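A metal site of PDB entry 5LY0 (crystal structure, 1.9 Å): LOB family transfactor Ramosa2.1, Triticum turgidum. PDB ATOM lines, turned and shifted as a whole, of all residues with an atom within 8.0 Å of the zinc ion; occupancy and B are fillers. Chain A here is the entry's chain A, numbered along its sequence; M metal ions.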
ATOM      1  N   ALA A  10      -0.318 -31.439  -2.470  1.00  0.00           N
ATOM      2  CA  ALA A  10      -0.604 -31.764  -3.856  1.00  0.00           C
ATOM      3  C   ALA A  10      -1.565 -30.735  -4.461  1.00  0.00           C
ATOM      4  O   ALA A  10      -2.599 -30.435  -3.862  1.00  0.00           O
ATOM      5  CB  ALA A  10      -1.193 -33.150  -3.967  1.00  0.00           C
ATOM      6  N   PRO A  11      -1.249 -30.208  -5.645  1.00  0.00           N
ATOM      7  CA  PRO A  11      -2.146 -29.231  -6.258  1.00  0.00           C
ATOM      8  C   PRO A  11      -3.379 -29.901  -6.840  1.00  0.00           C
ATOM      9  O   PRO A  11      -3.340 -31.060  -7.271  1.00  0.00           O
ATOM     10  CB  PRO A  11      -1.289 -28.609  -7.359  1.00  0.00           C
ATOM     11  CG  PRO A  11      -0.357 -29.698  -7.759  1.00  0.00           C
ATOM     12  CD  PRO A  11      -0.106 -30.519  -6.520  1.00  0.00           C
ATOM     13  N   CYS A  12      -4.492 -29.173  -6.844  1.00  0.00           N
ATOM     14  CA  CYS A  12      -5.693 -29.688  -7.468  1.00  0.00           C
ATOM     15  C   CYS A  12      -5.502 -29.760  -8.977  1.00  0.00           C
ATOM     16  O   CYS A  12      -4.563 -29.187  -9.547  1.00  0.00           O
ATOM     17  CB  CYS A  12      -6.903 -28.816  -7.122  1.00  0.00           C
ATOM     18  SG  CYS A  12      -7.005 -27.276  -8.060  1.00  0.00           S
ATOM     19  N   ALA A  13      -6.408 -30.488  -9.633  1.00  0.00           N
ATOM     20  CA  ALA A  13      -6.270 -30.709 -11.070  1.00  0.00           C
ATOM     21  C   ALA A  13      -6.321 -29.395 -11.847  1.00  0.00           C
ATOM     22  O   ALA A  13      -5.678 -29.268 -12.898  1.00  0.00           O
ATOM     23  CB  ALA A  13      -7.358 -31.654 -11.563  1.00  0.00           C
ATOM     24  N   ALA A  14      -7.076 -28.412 -11.365  1.00  0.00           N
ATOM     25  CA  ALA A  14      -7.163 -27.137 -12.057  1.00  0.00           C
ATOM     26  C   ALA A  14      -5.830 -26.405 -12.013  1.00  0.00           C
ATOM     27  O   ALA A  14      -5.340 -25.913 -13.044  1.00  0.00           O
ATOM     28  CB  ALA A  14      -8.264 -26.268 -11.435  1.00  0.00           C
ATOM     29  N   CYS A  15      -5.204 -26.339 -10.828  1.00  0.00           N
ATOM     30  CA  CYS A  15      -3.948 -25.617 -10.690  1.00  0.00           C
ATOM     31  C   CYS A  15      -2.806 -26.343 -11.398  1.00  0.00           C
ATOM     32  O   CYS A  15      -1.918 -25.709 -11.975  1.00  0.00           O
ATOM     33  CB  CYS A  15      -3.621 -25.407  -9.216  1.00  0.00           C
ATOM     34  SG  CYS A  15      -4.740 -24.237  -8.393  1.00  0.00           S
ATOM     35  N   LYS A  16      -2.813 -27.682 -11.374  1.00  0.00           N
ATOM     36  CA  LYS A  16      -1.818 -28.436 -12.126  1.00  0.00           C
ATOM     37  C   LYS A  16      -1.942 -28.134 -13.618  1.00  0.00           C
ATOM     38  O   LYS A  16      -0.938 -27.903 -14.305  1.00  0.00           O
ATOM     39  CB  LYS A  16      -1.966 -29.936 -11.872  1.00  0.00           C
ATOM     40  CG  LYS A  16      -1.033 -30.781 -12.728  1.00  0.00           C
ATOM     41  CD  LYS A  16      -0.955 -32.227 -12.262  1.00  0.00           C
ATOM     42  CE  LYS A  16       0.006 -33.026 -13.145  1.00  0.00           C
ATOM     43  NZ  LYS A  16      -0.163 -34.500 -12.977  1.00  0.00           N
ATOM     44  N   LEU A  18      -3.386 -25.421 -15.061  1.00  0.00           N
ATOM     45  CA  LEU A  18      -3.029 -24.024 -15.261  1.00  0.00           C
ATOM     46  C   LEU A  18      -1.593 -23.731 -14.858  1.00  0.00           C
ATOM     47  O   LEU A  18      -1.139 -22.593 -15.031  1.00  0.00           O
ATOM     48  CB  LEU A  18      -3.995 -23.125 -14.479  1.00  0.00           C
ATOM     49  CG  LEU A  18      -5.476 -23.303 -14.833  1.00  0.00           C
ATOM     50  CD1 LEU A  18      -6.364 -22.686 -13.769  1.00  0.00           C
ATOM     51  CD2 LEU A  18      -5.779 -22.708 -16.203  1.00  0.00           C
ATOM     52  N   ARG A  20      -0.159 -23.337 -11.967  1.00  0.00           N
ATOM     53  CA  ARG A  20      -0.062 -22.325 -10.921  1.00  0.00           C
ATOM     54  C   ARG A  20      -0.075 -22.998  -9.556  1.00  0.00           C
ATOM     55  O   ARG A  20      -0.426 -24.161  -9.420  1.00  0.00           O
ATOM     56  CB  ARG A  20      -1.205 -21.303 -11.022  1.00  0.00           C
ATOM     57  CG  ARG A  20      -2.566 -21.854 -10.676  1.00  0.00           C
ATOM     58  CD  ARG A  20      -3.641 -20.807 -10.911  1.00  0.00           C
ATOM     59  NE  ARG A  20      -4.868 -21.108 -10.175  1.00  0.00           N
ATOM     60  CZ  ARG A  20      -6.037 -20.535 -10.414  1.00  0.00           C
ATOM     61  NH1 ARG A  20      -6.168 -19.639 -11.376  1.00  0.00           N
ATOM     62  NH2 ARG A  20      -7.096 -20.868  -9.684  1.00  0.00           N
ATOM     63  N   LYS A  21       0.315 -22.215  -8.547  1.00  0.00           N
ATOM     64  CA  LYS A  21       0.384 -22.729  -7.187  1.00  0.00           C
ATOM     65  C   LYS A  21      -1.015 -22.867  -6.598  1.00  0.00           C
ATOM     66  O   LYS A  21      -1.794 -21.909  -6.600  1.00  0.00           O
ATOM     67  CB  LYS A  21       1.227 -21.786  -6.329  1.00  0.00           C
ATOM     68  CG  LYS A  21       1.658 -22.353  -4.980  1.00  0.00           C
ATOM     69  CD  LYS A  21       3.008 -23.037  -5.066  1.00  0.00           C
ATOM     70  CE  LYS A  21       3.561 -23.341  -3.686  1.00  0.00           C
ATOM     71  NZ  LYS A  21       2.605 -24.136  -2.872  1.00  0.00           N
ATOM     72  N   CYS A  22      -1.337 -24.068  -6.107  1.00  0.00           N
ATOM     73  CA  CYS A  22      -2.634 -24.322  -5.479  1.00  0.00           C
ATOM     74  C   CYS A  22      -2.532 -23.891  -4.021  1.00  0.00           C
ATOM     75  O   CYS A  22      -1.953 -24.594  -3.190  1.00  0.00           O
ATOM     76  CB  CYS A  22      -3.010 -25.793  -5.614  1.00  0.00           C
ATOM     77  SG  CYS A  22      -4.674 -26.192  -5.005  1.00  0.00           S
ATOM     78  N   LEU A  23      -3.101 -22.733  -3.703  1.00  0.00           N
ATOM     79  CA  LEU A  23      -2.970 -22.135  -2.397  1.00  0.00           C
ATOM     80  C   LEU A  23      -4.176 -22.459  -1.521  1.00  0.00           C
ATOM     81  O   LEU A  23      -5.254 -22.806  -2.026  1.00  0.00           O
ATOM     82  CB  LEU A  23      -2.824 -20.616  -2.521  1.00  0.00           C
ATOM     83  CG  LEU A  23      -1.549 -20.132  -3.202  1.00  0.00           C
ATOM     84  CD1 LEU A  23      -1.658 -18.654  -3.559  1.00  0.00           C
ATOM     85  CD2 LEU A  23      -0.341 -20.385  -2.316  1.00  0.00           C
ATOM     86  N   PRO A  24      -4.030 -22.365  -0.206  1.00  0.00           N
ATOM     87  CA  PRO A  24      -5.196 -22.471   0.678  1.00  0.00           C
ATOM     88  C   PRO A  24      -6.314 -21.544   0.227  1.00  0.00           C
ATOM     89  O   PRO A  24      -6.091 -20.362  -0.054  1.00  0.00           O
ATOM     90  CB  PRO A  24      -4.633 -22.066   2.047  1.00  0.00           C
ATOM     91  CG  PRO A  24      -3.188 -22.429   1.981  1.00  0.00           C
ATOM     92  CD  PRO A  24      -2.767 -22.220   0.543  1.00  0.00           C
ATOM     93  N   GLY A  25      -7.520 -22.088   0.157  1.00  0.00           N
ATOM     94  CA  GLY A  25      -8.665 -21.340  -0.314  1.00  0.00           C
ATOM     95  C   GLY A  25      -8.899 -21.418  -1.806  1.00  0.00           C
ATOM     96  O   GLY A  25      -9.835 -20.762  -2.296  1.00  0.00           O
ATOM     97  N   CYS A  26      -8.102 -22.182  -2.538  1.00  0.00           N
ATOM     98  CA  CYS A  26      -8.316 -22.370  -3.966  1.00  0.00           C
ATOM     99  C   CYS A  26      -9.779 -22.696  -4.252  1.00  0.00           C
ATOM    100  O   CYS A  26     -10.358 -23.590  -3.620  1.00  0.00           O
ATOM    101  CB  CYS A  26      -7.415 -23.487  -4.492  1.00  0.00           C
ATOM    102  SG  CYS A  26      -7.682 -23.880  -6.232  1.00  0.00           S
ATOM    103  N   VAL A  27     -10.377 -21.964  -5.199  1.00  0.00           N
ATOM    104  CA  VAL A  27     -11.796 -22.145  -5.481  1.00  0.00           C
ATOM    105  C   VAL A  27     -12.069 -23.458  -6.205  1.00  0.00           C
ATOM    106  O   VAL A  27     -13.197 -23.969  -6.148  1.00  0.00           O
ATOM    107  CB  VAL A  27     -12.346 -20.963  -6.308  1.00  0.00           C
ATOM    108  CG1 VAL A  27     -12.275 -19.665  -5.506  1.00  0.00           C
ATOM    109  CG2 VAL A  27     -11.598 -20.832  -7.638  1.00  0.00           C
ATOM    110  N   PHE A  28     -11.074 -24.024  -6.890  1.00  0.00           N
ATOM    111  CA  PHE A  28     -11.277 -25.264  -7.631  1.00  0.00           C
ATOM    112  C   PHE A  28     -11.014 -26.507  -6.786  1.00  0.00           C
ATOM    113  O   PHE A  28     -11.595 -27.564  -7.064  1.00  0.00           O
ATOM    114  CB  PHE A  28     -10.347 -25.329  -8.851  1.00  0.00           C
ATOM    115  CG  PHE A  28     -10.590 -24.247  -9.855  1.00  0.00           C
ATOM    116  CD1 PHE A  28     -11.763 -24.204 -10.585  1.00  0.00           C
ATOM    117  CD2 PHE A  28      -9.621 -23.290 -10.105  1.00  0.00           C
ATOM    118  CE1 PHE A  28     -11.980 -23.208 -11.526  1.00  0.00           C
ATOM    119  CE2 PHE A  28      -9.830 -22.300 -11.049  1.00  0.00           C
ATOM    120  CZ  PHE A  28     -11.012 -22.263 -11.757  1.00  0.00           C
ATOM    121  N   ALA A  29     -10.159 -26.405  -5.778  1.00  0.00           N
ATOM    122  CA  ALA A  29      -9.630 -27.598  -5.118  1.00  0.00           C
ATOM    123  C   ALA A  29     -10.711 -28.518  -4.559  1.00  0.00           C
ATOM    124  O   ALA A  29     -10.558 -29.748  -4.695  1.00  0.00           O
ATOM    125  CB  ALA A  29      -8.651 -27.186  -4.015  1.00  0.00           C
ATOM    126  N   PRO A  30     -11.795 -28.043  -3.943  1.00  0.00           N
ATOM    127  CA  PRO A  30     -12.785 -28.971  -3.389  1.00  0.00           C
ATOM    128  C   PRO A  30     -13.486 -29.813  -4.429  1.00  0.00           C
ATOM    129  O   PRO A  30     -14.105 -30.822  -4.074  1.00  0.00           O
ATOM    130  CB  PRO A  30     -13.774 -28.049  -2.664  1.00  0.00           C
ATOM    131  CG  PRO A  30     -13.050 -26.770  -2.464  1.00  0.00           C
ATOM    132  CD  PRO A  30     -12.135 -26.639  -3.635  1.00  0.00           C
ATOM    133  N   PHE A  32     -12.190 -30.373  -8.025  1.00  0.00           N
ATOM    134  CA  PHE A  32     -11.365 -30.906  -9.109  1.00  0.00           C
ATOM    135  C   PHE A  32     -10.160 -31.608  -8.487  1.00  0.00           C
ATOM    136  O   PHE A  32      -9.051 -31.060  -8.474  1.00  0.00           O
ATOM    137  CB  PHE A  32     -10.942 -29.803 -10.079  1.00  0.00           C
ATOM    138  CG  PHE A  32     -12.076 -29.239 -10.884  1.00  0.00           C
ATOM    139  CD1 PHE A  32     -12.504 -29.871 -12.039  1.00  0.00           C
ATOM    140  CD2 PHE A  32     -12.709 -28.079 -10.500  1.00  0.00           C
ATOM    141  CE1 PHE A  32     -13.547 -29.365 -12.790  1.00  0.00           C
ATOM    142  CE2 PHE A  32     -13.750 -27.557 -11.246  1.00  0.00           C
ATOM    143  CZ  PHE A  32     -14.169 -28.200 -12.391  1.00  0.00           C
HETATM  144 ZN    ZN M   1      -6.037 -25.452  -6.832  1.00  0.00          ZN
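The backbone NH of Ala 29 sits close to the side-chain sulfur of Cys 26, 3.6 Å away. The side-chain sulfur (SG) of Cys 26 lies close to the backbone NH (N) of Phe 28, 3.5 Å away. The backbone carbonyl oxygen of Cys 15 sits at hydrogen-bond distance from the backbone NH of Arg 20 (3.0 Å). The side-chain sulfur of Cys 12 lies close to the backbone NH of Ala 14 (3.5 Å).
Within 4 Å of the zinc ion: Cys 12, Cys 15, Cys 22 and Cys 26.
SG of Cys 26 binds the zinc ion (2.4 Å). The side-chain sulfur (SG) of Cys 15 binds the zinc ion (2.4 Å). The zinc ion is bound by SG of Cys 22 (2.4 Å). The zinc ion is bound by the side-chain sulfur (SG) of Cys 12. The zinc ion has four donor atoms within binding distance.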
